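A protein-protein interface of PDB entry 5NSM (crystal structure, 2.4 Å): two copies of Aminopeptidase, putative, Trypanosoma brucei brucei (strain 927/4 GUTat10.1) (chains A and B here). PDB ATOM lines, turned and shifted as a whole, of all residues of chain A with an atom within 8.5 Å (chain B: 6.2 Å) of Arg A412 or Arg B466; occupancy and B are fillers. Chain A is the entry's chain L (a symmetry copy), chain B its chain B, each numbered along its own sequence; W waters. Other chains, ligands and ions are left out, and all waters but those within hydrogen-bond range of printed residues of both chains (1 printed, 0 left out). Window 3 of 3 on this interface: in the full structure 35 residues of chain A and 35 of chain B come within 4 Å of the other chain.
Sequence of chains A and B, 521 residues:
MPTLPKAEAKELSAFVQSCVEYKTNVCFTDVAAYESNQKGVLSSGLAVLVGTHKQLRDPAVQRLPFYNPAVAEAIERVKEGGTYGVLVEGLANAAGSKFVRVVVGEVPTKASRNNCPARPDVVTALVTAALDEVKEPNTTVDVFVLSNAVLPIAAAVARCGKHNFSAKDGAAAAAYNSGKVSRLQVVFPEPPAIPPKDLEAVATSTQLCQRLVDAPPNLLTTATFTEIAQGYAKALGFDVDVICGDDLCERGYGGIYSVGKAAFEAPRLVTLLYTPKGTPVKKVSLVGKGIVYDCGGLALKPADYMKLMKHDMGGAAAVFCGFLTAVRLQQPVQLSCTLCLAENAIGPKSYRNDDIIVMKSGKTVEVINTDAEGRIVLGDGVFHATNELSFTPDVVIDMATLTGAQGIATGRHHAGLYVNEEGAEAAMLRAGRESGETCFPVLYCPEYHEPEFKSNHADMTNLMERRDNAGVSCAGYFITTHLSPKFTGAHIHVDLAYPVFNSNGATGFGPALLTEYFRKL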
ATOM      1  N   LEU A 308     -16.169 -37.494  13.225  1.00  0.00           N
ATOM      2  CA  LEU A 308     -16.021 -37.707  11.744  1.00  0.00           C
ATOM      3  C   LEU A 308     -14.553 -37.775  11.257  1.00  0.00           C
ATOM      4  O   LEU A 308     -14.295 -37.770  10.060  1.00  0.00           O
ATOM      5  CB  LEU A 308     -16.815 -36.671  10.917  1.00  0.00           C
ATOM      6  CG  LEU A 308     -18.330 -36.586  11.229  1.00  0.00           C
ATOM      7  CD1 LEU A 308     -18.997 -35.547  10.335  1.00  0.00           C
ATOM      8  CD2 LEU A 308     -19.073 -37.921  11.108  1.00  0.00           C
ATOM      9  N   GLN A 406      -9.092 -26.257   2.965  1.00  0.00           N
ATOM     10  CA  GLN A 406      -9.706 -26.715   1.710  1.00  0.00           C
ATOM     11  C   GLN A 406     -11.186 -26.322   1.591  1.00  0.00           C
ATOM     12  O   GLN A 406     -11.631 -25.868   0.540  1.00  0.00           O
ATOM     13  CB  GLN A 406      -9.559 -28.227   1.543  1.00  0.00           C
ATOM     14  CG  GLN A 406     -10.103 -28.770   0.217  1.00  0.00           C
ATOM     15  CD  GLN A 406     -11.563 -29.161   0.286  1.00  0.00           C
ATOM     16  OE1 GLN A 406     -11.947 -30.010   1.084  1.00  0.00           O
ATOM     17  NE2 GLN A 406     -12.395 -28.514  -0.530  1.00  0.00           N
ATOM     18  N   GLY A 407     -11.935 -26.519   2.667  1.00  0.00           N
ATOM     19  CA  GLY A 407     -13.358 -26.160   2.694  1.00  0.00           C
ATOM     20  C   GLY A 407     -13.616 -24.652   2.581  1.00  0.00           C
ATOM     21  O   GLY A 407     -14.425 -24.196   1.792  1.00  0.00           O
ATOM     22  N   ILE A 408     -12.831 -23.899   3.317  1.00  0.00           N
ATOM     23  CA  ILE A 408     -12.834 -22.442   3.245  1.00  0.00           C
ATOM     24  C   ILE A 408     -12.487 -21.929   1.839  1.00  0.00           C
ATOM     25  O   ILE A 408     -13.058 -20.971   1.340  1.00  0.00           O
ATOM     26  CB  ILE A 408     -11.884 -21.855   4.315  1.00  0.00           C
ATOM     27  CG1 ILE A 408     -12.524 -22.031   5.690  1.00  0.00           C
ATOM     28  CG2 ILE A 408     -11.632 -20.377   4.091  1.00  0.00           C
ATOM     29  CD1 ILE A 408     -11.544 -21.991   6.834  1.00  0.00           C
ATOM     30  N   ALA A 409     -11.522 -22.581   1.218  1.00  0.00           N
ATOM     31  CA  ALA A 409     -11.015 -22.159  -0.107  1.00  0.00           C
ATOM     32  C   ALA A 409     -11.958 -22.540  -1.266  1.00  0.00           C
ATOM     33  O   ALA A 409     -12.387 -21.686  -2.035  1.00  0.00           O
ATOM     34  CB  ALA A 409      -9.613 -22.710  -0.355  1.00  0.00           C
ATOM     35  N   THR A 410     -12.181 -23.828  -1.420  1.00  0.00           N
ATOM     36  CA  THR A 410     -12.909 -24.373  -2.589  1.00  0.00           C
ATOM     37  C   THR A 410     -14.254 -25.033  -2.273  1.00  0.00           C
ATOM     38  O   THR A 410     -14.979 -25.445  -3.163  1.00  0.00           O
ATOM     39  CB  THR A 410     -12.056 -25.379  -3.399  1.00  0.00           C
ATOM     40  OG1 THR A 410     -11.767 -26.527  -2.627  1.00  0.00           O
ATOM     41  CG2 THR A 410     -10.751 -24.759  -3.856  1.00  0.00           C
ATOM     42  N   GLY A 411     -14.552 -25.173  -0.991  1.00  0.00           N
ATOM     43  CA  GLY A 411     -15.884 -25.595  -0.558  1.00  0.00           C
ATOM     44  C   GLY A 411     -16.124 -27.084  -0.448  1.00  0.00           C
ATOM     45  O   GLY A 411     -15.229 -27.917  -0.625  1.00  0.00           O
ATOM     46  N   ARG A 412     -17.381 -27.417  -0.253  1.00  0.00           N
ATOM     47  CA  ARG A 412     -17.770 -28.810   0.023  1.00  0.00           C
ATOM     48  C   ARG A 412     -17.905 -29.748  -1.146  1.00  0.00           C
ATOM     49  O   ARG A 412     -17.904 -30.948  -0.954  1.00  0.00           O
ATOM     50  CB  ARG A 412     -19.057 -28.823   0.825  1.00  0.00           C
ATOM     51  CG  ARG A 412     -18.835 -28.067   2.108  1.00  0.00           C
ATOM     52  CD  ARG A 412     -19.805 -28.491   3.137  1.00  0.00           C
ATOM     53  NE  ARG A 412     -19.502 -27.917   4.443  1.00  0.00           N
ATOM     54  CZ  ARG A 412     -19.754 -28.533   5.588  1.00  0.00           C
ATOM     55  NH1 ARG A 412     -20.244 -29.766   5.594  1.00  0.00           N
ATOM     56  NH2 ARG A 412     -19.481 -27.924   6.731  1.00  0.00           N
ATOM     57  N   HIS A 413     -18.026 -29.197  -2.335  1.00  0.00           N
ATOM     58  CA  HIS A 413     -18.230 -30.012  -3.553  1.00  0.00           C
ATOM     59  C   HIS A 413     -17.049 -30.056  -4.487  1.00  0.00           C
ATOM     60  O   HIS A 413     -17.058 -30.796  -5.439  1.00  0.00           O
ATOM     61  CB  HIS A 413     -19.446 -29.519  -4.331  1.00  0.00           C
ATOM     62  CG  HIS A 413     -20.677 -29.414  -3.494  1.00  0.00           C
ATOM     63  ND1 HIS A 413     -20.975 -28.287  -2.752  1.00  0.00           N
ATOM     64  CD2 HIS A 413     -21.670 -30.300  -3.249  1.00  0.00           C
ATOM     65  CE1 HIS A 413     -22.099 -28.482  -2.088  1.00  0.00           C
ATOM     66  NE2 HIS A 413     -22.536 -29.696  -2.368  1.00  0.00           N
ATOM     67  N   HIS A 414     -16.056 -29.218  -4.228  1.00  0.00           N
ATOM     68  CA  HIS A 414     -14.875 -29.112  -5.109  1.00  0.00           C
ATOM     69  C   HIS A 414     -13.609 -29.438  -4.334  1.00  0.00           C
ATOM     70  O   HIS A 414     -13.223 -28.693  -3.445  1.00  0.00           O
ATOM     71  CB  HIS A 414     -14.755 -27.720  -5.724  1.00  0.00           C
ATOM     72  CG  HIS A 414     -15.777 -27.417  -6.785  1.00  0.00           C
ATOM     73  ND1 HIS A 414     -17.082 -27.096  -6.490  1.00  0.00           N
ATOM     74  CD2 HIS A 414     -15.670 -27.357  -8.135  1.00  0.00           C
ATOM     75  CE1 HIS A 414     -17.739 -26.876  -7.611  1.00  0.00           C
ATOM     76  NE2 HIS A 414     -16.903 -27.010  -8.624  1.00  0.00           N
ATOM     77  N   ALA A 415     -12.961 -30.525  -4.711  1.00  0.00           N
ATOM     78  CA  ALA A 415     -11.628 -30.839  -4.198  1.00  0.00           C
ATOM     79  C   ALA A 415     -10.623 -29.770  -4.690  1.00  0.00           C
ATOM     80  O   ALA A 415     -10.705 -29.306  -5.828  1.00  0.00           O
ATOM     81  CB  ALA A 415     -11.169 -32.213  -4.620  1.00  0.00           C
ATOM     82  N   THR A 438     -16.133 -32.989  -8.979  1.00  0.00           N
ATOM     83  CA  THR A 438     -15.547 -31.716  -9.389  1.00  0.00           C
ATOM     84  C   THR A 438     -14.372 -31.272  -8.506  1.00  0.00           C
ATOM     85  O   THR A 438     -14.312 -31.570  -7.293  1.00  0.00           O
ATOM     86  CB  THR A 438     -16.591 -30.597  -9.370  1.00  0.00           C
ATOM     87  OG1 THR A 438     -17.316 -30.658  -8.138  1.00  0.00           O
ATOM     88  CG2 THR A 438     -17.549 -30.755 -10.500  1.00  0.00           C
ATOM     89  N   LEU A 496      -9.163 -33.375  -0.746  1.00  0.00           N
ATOM     90  CA  LEU A 496     -10.599 -33.706  -0.761  1.00  0.00           C
ATOM     91  C   LEU A 496     -11.196 -33.835   0.651  1.00  0.00           C
ATOM     92  O   LEU A 496     -12.076 -34.653   0.914  1.00  0.00           O
ATOM     93  CB  LEU A 496     -10.883 -34.962  -1.593  1.00  0.00           C
ATOM     94  CG  LEU A 496      -9.836 -36.060  -1.602  1.00  0.00           C
ATOM     95  CD1 LEU A 496      -9.657 -36.709  -0.256  1.00  0.00           C
ATOM     96  CD2 LEU A 496     -10.210 -37.112  -2.629  1.00  0.00           C
ATOM     97  N   ALA A 497     -10.741 -32.968   1.538  1.00  0.00           N
ATOM     98  CA  ALA A 497     -11.168 -32.989   2.966  1.00  0.00           C
ATOM     99  C   ALA A 497     -12.700 -33.012   3.114  1.00  0.00           C
ATOM    100  O   ALA A 497     -13.239 -33.833   3.779  1.00  0.00           O
ATOM    101  CB  ALA A 497     -10.584 -31.792   3.721  1.00  0.00           C
ATOM    102  N   TYR A 498     -13.356 -32.097   2.435  1.00  0.00           N
ATOM    103  CA  TYR A 498     -14.819 -31.967   2.507  1.00  0.00           C
ATOM    104  C   TYR A 498     -15.641 -32.769   1.475  1.00  0.00           C
ATOM    105  O   TYR A 498     -16.705 -33.277   1.818  1.00  0.00           O
ATOM    106  CB  TYR A 498     -15.256 -30.501   2.503  1.00  0.00           C
ATOM    107  CG  TYR A 498     -14.941 -29.823   3.803  1.00  0.00           C
ATOM    108  CD1 TYR A 498     -13.693 -29.254   4.025  1.00  0.00           C
ATOM    109  CD2 TYR A 498     -15.874 -29.779   4.838  1.00  0.00           C
ATOM    110  CE1 TYR A 498     -13.378 -28.665   5.233  1.00  0.00           C
ATOM    111  CE2 TYR A 498     -15.573 -29.167   6.045  1.00  0.00           C
ATOM    112  CZ  TYR A 498     -14.323 -28.612   6.230  1.00  0.00           C
ATOM    113  OH  TYR A 498     -14.003 -28.011   7.425  1.00  0.00           O
ATOM    114  N   PRO A 499     -15.166 -32.885   0.224  1.00  0.00           N
ATOM    115  CA  PRO A 499     -16.000 -33.581  -0.775  1.00  0.00           C
ATOM    116  C   PRO A 499     -16.224 -35.079  -0.525  1.00  0.00           C
ATOM    117  O   PRO A 499     -17.138 -35.643  -1.081  1.00  0.00           O
ATOM    118  CB  PRO A 499     -15.209 -33.391  -2.060  1.00  0.00           C
ATOM    119  CG  PRO A 499     -14.460 -32.140  -1.857  1.00  0.00           C
ATOM    120  CD  PRO A 499     -14.135 -32.061  -0.408  1.00  0.00           C
ATOM    121  N   VAL A 500     -15.424 -35.670   0.362  1.00  0.00           N
ATOM    122  CA  VAL A 500     -15.591 -37.086   0.733  1.00  0.00           C
ATOM    123  C   VAL A 500     -16.787 -37.399   1.661  1.00  0.00           C
ATOM    124  O   VAL A 500     -17.071 -38.536   1.905  1.00  0.00           O
ATOM    125  CB  VAL A 500     -14.360 -37.718   1.360  1.00  0.00           C
ATOM    126  CG1 VAL A 500     -13.213 -37.644   0.368  1.00  0.00           C
ATOM    127  CG2 VAL A 500     -14.024 -37.064   2.693  1.00  0.00           C
ATOM    128  N   PHE A 501     -17.471 -36.385   2.137  1.00  0.00           N
ATOM    129  CA  PHE A 501     -18.631 -36.607   2.993  1.00  0.00           C
ATOM    130  C   PHE A 501     -19.696 -35.527   2.854  1.00  0.00           C
ATOM    131  O   PHE A 501     -19.433 -34.438   2.411  1.00  0.00           O
ATOM    132  CB  PHE A 501     -18.218 -36.773   4.477  1.00  0.00           C
ATOM    133  CG  PHE A 501     -17.906 -35.463   5.190  1.00  0.00           C
ATOM    134  CD1 PHE A 501     -16.650 -34.880   5.074  1.00  0.00           C
ATOM    135  CD2 PHE A 501     -18.853 -34.859   6.010  1.00  0.00           C
ATOM    136  CE1 PHE A 501     -16.361 -33.691   5.706  1.00  0.00           C
ATOM    137  CE2 PHE A 501     -18.566 -33.689   6.671  1.00  0.00           C
ATOM    138  CZ  PHE A 501     -17.320 -33.090   6.506  1.00  0.00           C
ATOM    139  N   ASN A 502     -20.902 -35.890   3.232  1.00  0.00           N
ATOM    140  CA  ASN A 502     -21.967 -34.914   3.442  1.00  0.00           C
ATOM    141  C   ASN A 502     -22.715 -35.290   4.729  1.00  0.00           C
ATOM    142  O   ASN A 502     -22.267 -36.133   5.477  1.00  0.00           O
ATOM    143  CB  ASN A 502     -22.882 -34.811   2.230  1.00  0.00           C
ATOM    144  CG  ASN A 502     -23.616 -36.099   1.941  1.00  0.00           C
ATOM    145  OD1 ASN A 502     -23.875 -36.910   2.825  1.00  0.00           O
ATOM    146  ND2 ASN A 502     -23.979 -36.282   0.702  1.00  0.00           N
ATOM    147  N   SER A 503     -23.856 -34.677   4.977  1.00  0.00           N
ATOM    148  CA  SER A 503     -24.594 -34.891   6.252  1.00  0.00           C
ATOM    149  C   SER A 503     -25.149 -36.315   6.395  1.00  0.00           C
ATOM    150  O   SER A 503     -25.470 -36.742   7.487  1.00  0.00           O
ATOM    151  CB  SER A 503     -25.725 -33.878   6.431  1.00  0.00           C
ATOM    152  OG  SER A 503     -26.683 -34.070   5.416  1.00  0.00           O
ATOM    153  N   THR A 507     -19.452 -39.913   0.695  1.00  0.00           N
ATOM    154  CA  THR A 507     -19.921 -39.722  -0.685  1.00  0.00           C
ATOM    155  C   THR A 507     -19.308 -40.691  -1.707  1.00  0.00           C
ATOM    156  O   THR A 507     -19.788 -40.801  -2.811  1.00  0.00           O
ATOM    157  CB  THR A 507     -19.608 -38.309  -1.201  1.00  0.00           C
ATOM    158  OG1 THR A 507     -18.191 -38.086  -1.109  1.00  0.00           O
ATOM    159  CG2 THR A 507     -20.375 -37.263  -0.430  1.00  0.00           C
ATOM    160  N   PHE A 509     -16.419 -40.071  -3.078  1.00  0.00           N
ATOM    161  CA  PHE A 509     -15.785 -39.123  -3.996  1.00  0.00           C
ATOM    162  C   PHE A 509     -14.348 -39.556  -4.209  1.00  0.00           C
ATOM    163  O   PHE A 509     -13.625 -39.865  -3.256  1.00  0.00           O
ATOM    164  CB  PHE A 509     -15.830 -37.720  -3.399  1.00  0.00           C
ATOM    165  CG  PHE A 509     -15.221 -36.655  -4.252  1.00  0.00           C
ATOM    166  CD1 PHE A 509     -13.829 -36.522  -4.359  1.00  0.00           C
ATOM    167  CD2 PHE A 509     -16.025 -35.720  -4.886  1.00  0.00           C
ATOM    168  CE1 PHE A 509     -13.267 -35.518  -5.130  1.00  0.00           C
ATOM    169  CE2 PHE A 509     -15.466 -34.703  -5.651  1.00  0.00           C
ATOM    170  CZ  PHE A 509     -14.085 -34.599  -5.770  1.00  0.00           C
ATOM    171  N   TYR B 448     -23.946 -23.265  -5.950  1.00  0.00           N
ATOM    172  CA  TYR B 448     -23.515 -23.786  -4.650  1.00  0.00           C
ATOM    173  C   TYR B 448     -23.381 -22.733  -3.558  1.00  0.00           C
ATOM    174  O   TYR B 448     -23.427 -23.051  -2.389  1.00  0.00           O
ATOM    175  CB  TYR B 448     -22.227 -24.574  -4.742  1.00  0.00           C
ATOM    176  CG  TYR B 448     -22.302 -25.848  -5.519  1.00  0.00           C
ATOM    177  CD1 TYR B 448     -23.523 -26.464  -5.813  1.00  0.00           C
ATOM    178  CD2 TYR B 448     -21.144 -26.480  -5.926  1.00  0.00           C
ATOM    179  CE1 TYR B 448     -23.587 -27.650  -6.532  1.00  0.00           C
ATOM    180  CE2 TYR B 448     -21.192 -27.676  -6.632  1.00  0.00           C
ATOM    181  CZ  TYR B 448     -22.424 -28.260  -6.934  1.00  0.00           C
ATOM    182  OH  TYR B 448     -22.455 -29.448  -7.651  1.00  0.00           O
ATOM    183  N   GLU B 452     -26.351 -21.026   0.883  1.00  0.00           N
ATOM    184  CA  GLU B 452     -25.723 -20.609   2.148  1.00  0.00           C
ATOM    185  C   GLU B 452     -26.355 -19.377   2.779  1.00  0.00           C
ATOM    186  O   GLU B 452     -26.142 -19.090   3.939  1.00  0.00           O
ATOM    187  CB  GLU B 452     -24.215 -20.393   1.967  1.00  0.00           C
ATOM    188  CG  GLU B 452     -23.465 -21.679   1.663  1.00  0.00           C
ATOM    189  CD  GLU B 452     -23.500 -22.689   2.818  1.00  0.00           C
ATOM    190  OE1 GLU B 452     -23.772 -22.282   3.953  1.00  0.00           O
ATOM    191  OE2 GLU B 452     -23.258 -23.894   2.578  1.00  0.00           O
ATOM    192  N   LEU B 463     -24.601 -13.722   5.970  1.00  0.00           N
ATOM    193  CA  LEU B 463     -23.550 -14.644   6.393  1.00  0.00           C
ATOM    194  C   LEU B 463     -23.855 -16.075   5.999  1.00  0.00           C
ATOM    195  O   LEU B 463     -24.972 -16.524   6.097  1.00  0.00           O
ATOM    196  CB  LEU B 463     -23.351 -14.556   7.896  1.00  0.00           C
ATOM    197  CG  LEU B 463     -22.040 -15.155   8.450  1.00  0.00           C
ATOM    198  CD1 LEU B 463     -20.885 -14.177   8.282  1.00  0.00           C
ATOM    199  CD2 LEU B 463     -22.194 -15.523   9.920  1.00  0.00           C
ATOM    200  N   MET B 464     -22.825 -16.771   5.549  1.00  0.00           N
ATOM    201  CA  MET B 464     -22.954 -18.191   5.182  1.00  0.00           C
ATOM    202  C   MET B 464     -23.315 -19.001   6.430  1.00  0.00           C
ATOM    203  O   MET B 464     -22.839 -18.784   7.519  1.00  0.00           O
ATOM    204  CB  MET B 464     -21.754 -18.801   4.428  1.00  0.00           C
ATOM    205  CG  MET B 464     -20.406 -18.213   4.740  1.00  0.00           C
ATOM    206  SD  MET B 464     -19.099 -18.292   3.503  1.00  0.00           S
ATOM    207  CE  MET B 464     -18.961 -20.005   3.027  1.00  0.00           C
ATOM    208  N   GLU B 465     -24.266 -19.876   6.230  1.00  0.00           N
ATOM    209  CA  GLU B 465     -24.690 -20.859   7.229  1.00  0.00           C
ATOM    210  C   GLU B 465     -23.512 -21.774   7.628  1.00  0.00           C
ATOM    211  O   GLU B 465     -23.316 -22.075   8.783  1.00  0.00           O
ATOM    212  CB  GLU B 465     -25.864 -21.654   6.644  1.00  0.00           C
ATOM    213  CG  GLU B 465     -26.114 -23.019   7.228  1.00  0.00           C
ATOM    214  CD  GLU B 465     -27.272 -23.019   8.187  1.00  0.00           C
ATOM    215  OE1 GLU B 465     -28.364 -23.456   7.753  1.00  0.00           O
ATOM    216  OE2 GLU B 465     -27.083 -22.562   9.350  1.00  0.00           O
ATOM    217  N   ARG B 466     -22.779 -22.230   6.627  1.00  0.00           N
ATOM    218  CA  ARG B 466     -21.601 -23.096   6.804  1.00  0.00           C
ATOM    219  C   ARG B 466     -20.360 -22.336   6.300  1.00  0.00           C
ATOM    220  O   ARG B 466     -20.188 -22.140   5.111  1.00  0.00           O
ATOM    221  CB  ARG B 466     -21.758 -24.425   6.072  1.00  0.00           C
ATOM    222  CG  ARG B 466     -23.000 -25.211   6.464  1.00  0.00           C
ATOM    223  CD  ARG B 466     -23.194 -26.499   5.678  1.00  0.00           C
ATOM    224  NE  ARG B 466     -23.382 -26.248   4.252  1.00  0.00           N
ATOM    225  CZ  ARG B 466     -23.490 -27.185   3.313  1.00  0.00           C
ATOM    226  NH1 ARG B 466     -23.444 -28.476   3.622  1.00  0.00           N
ATOM    227  NH2 ARG B 466     -23.631 -26.832   2.034  1.00  0.00           N
ATOM    228  N   ARG B 467     -19.536 -21.897   7.239  1.00  0.00           N
ATOM    229  CA  ARG B 467     -18.373 -21.021   6.990  1.00  0.00           C
ATOM    230  C   ARG B 467     -17.335 -21.720   6.128  1.00  0.00           C
ATOM    231  O   ARG B 467     -16.566 -21.103   5.408  1.00  0.00           O
ATOM    232  CB  ARG B 467     -17.765 -20.557   8.326  1.00  0.00           C
ATOM    233  N   ASP B 468     -17.366 -23.039   6.148  1.00  0.00           N
ATOM    234  CA  ASP B 468     -16.364 -23.862   5.419  1.00  0.00           C
ATOM    235  C   ASP B 468     -16.849 -24.345   4.038  1.00  0.00           C
ATOM    236  O   ASP B 468     -16.560 -25.461   3.604  1.00  0.00           O
ATOM    237  CB  ASP B 468     -15.858 -25.026   6.271  1.00  0.00           C
ATOM    238  CG  ASP B 468     -16.976 -25.833   6.912  1.00  0.00           C
ATOM    239  OD1 ASP B 468     -18.148 -25.760   6.455  1.00  0.00           O
ATOM    240  OD2 ASP B 468     -16.663 -26.548   7.874  1.00  0.00           O
ATOM    241  N   ASN B 469     -17.528 -23.454   3.331  1.00  0.00           N
ATOM    242  CA  ASN B 469     -18.055 -23.737   1.975  1.00  0.00           C
ATOM    243  C   ASN B 469     -17.744 -22.625   0.954  1.00  0.00           C
ATOM    244  O   ASN B 469     -18.646 -22.017   0.393  1.00  0.00           O
ATOM    245  CB  ASN B 469     -19.557 -23.993   2.022  1.00  0.00           C
ATOM    246  CG  ASN B 469     -20.084 -24.637   0.745  1.00  0.00           C
ATOM    247  OD1 ASN B 469     -19.341 -25.238  -0.023  1.00  0.00           O
ATOM    248  ND2 ASN B 469     -21.375 -24.547   0.550  1.00  0.00           N
ATOM    249  N   ALA B 470     -16.455 -22.399   0.745  1.00  0.00           N
ATOM    250  CA  ALA B 470     -15.923 -21.417  -0.251  1.00  0.00           C
ATOM    251  C   ALA B 470     -16.229 -19.997   0.203  1.00  0.00           C
ATOM    252  O   ALA B 470     -17.088 -19.303  -0.337  1.00  0.00           O
ATOM    253  CB  ALA B 470     -16.467 -21.681  -1.657  1.00  0.00           C
ATOM    254  N   CYS B 474     -18.400 -17.034  -1.625  1.00  0.00           N
ATOM    255  CA  CYS B 474     -19.750 -16.703  -1.110  1.00  0.00           C
ATOM    256  C   CYS B 474     -19.961 -15.220  -0.822  1.00  0.00           C
ATOM    257  O   CYS B 474     -21.023 -14.670  -1.092  1.00  0.00           O
ATOM    258  CB  CYS B 474     -20.112 -17.530   0.118  1.00  0.00           C
ATOM    259  SG  CYS B 474     -20.551 -19.247  -0.267  1.00  0.00           S
HETATM  260  O   HOH W   1     -19.822 -25.231  -2.688  1.00  0.00           O
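The backbone carbonyl oxygen (O) of Gly A407 is in hydrogen-bond range of the backbone NH (N) of Ala B470 (2.9 Å). O of Gly A407 sits close to O of Asp B468 (3.1 Å). The side-chain carboxylate of Asp B468 sits at hydrogen-bond distance from the side-chain hydroxyl of Tyr A498. N of Arg A412 sits at hydrogen-bond distance from OD1 of Asn B469 (2.9 Å). NH2 of Arg A412 lies within salt-bridge range of OD1 of Asp B468 (2.6 Å).
The side-chain hydroxyl of Thr A438 is in hydrogen-bond range of the backbone carbonyl oxygen of His A413, 2.7 Å away. The side-chain hydroxyl (OG1) of Thr A410 lies within hydrogen-bond range of the backbone carbonyl oxygen (O) of His A414. The backbone carbonyl oxygen (O) of Gly A411 is in hydrogen-bond range of the side-chain amide nitrogen (NE2) of Gln A406 (2.9 Å). The side-chain amide nitrogen of Asn B469 is in hydrogen-bond range of the side-chain carboxylate of Glu B452 (2.8 Å). NE2 of Gln A406 is in hydrogen-bond range of O of His A414 (3.0 Å). The backbone NH (N) of Tyr A498 lies within hydrogen-bond range of the side-chain amide oxygen (OE1) of Gln A406 (2.9 Å).
Among the printed residues, merely in contact across the chains: Gly A407 with Asn B469, Ile A408 with Ala B470, Ala A409 with Ala B470, Gly A411 with Asn B469, Gly A411 with Ala B470, Arg A412 with Arg B466, His A413 with Tyr B448 and His A414 with Tyr B448.
Of the printed residues of chain B, Ala A409 touches Ala B470 (3.97 Å). Arg A412 touches just these residues of chain B: Arg B466 (3.7 Å), Asp B468 (2.6 Å) and Asn B469 (2.9 Å). No residue of chain A comes within 4 Å of Arg B467. Of the printed residues of chain A, Asn B469 touches Gly A407 (3.5 Å), Gly A411 (3.5 Å) and Arg A412 (2.9 Å). Printed residues of chain A within 4 Å of Ala B470: Gly A407, Ile A408, Ala A409 and Gly A411. The nearest residue of chain A that does not touch Arg B466 is His A413 (4.7 Å).
Hydrophobic or aromatic side chains of chain B that line the printed part of chain A: Tyr B448. Hydrophobic or aromatic side chains of chain A within 4 Å of the printed part of chain B: His A413, His A414 and Tyr A498. Among the printed residues, Asp or Glu carboxylates within 4 Å of a Lys or Arg side-chain nitrogen of the other chain: Arg A412 with Asp B468.
No position is printed for both chains.
Water W1 lies within hydrogen-bond range of OD1 of Asn B469 (2.7 Å) and ND1 of His A413 (3.3 Å).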
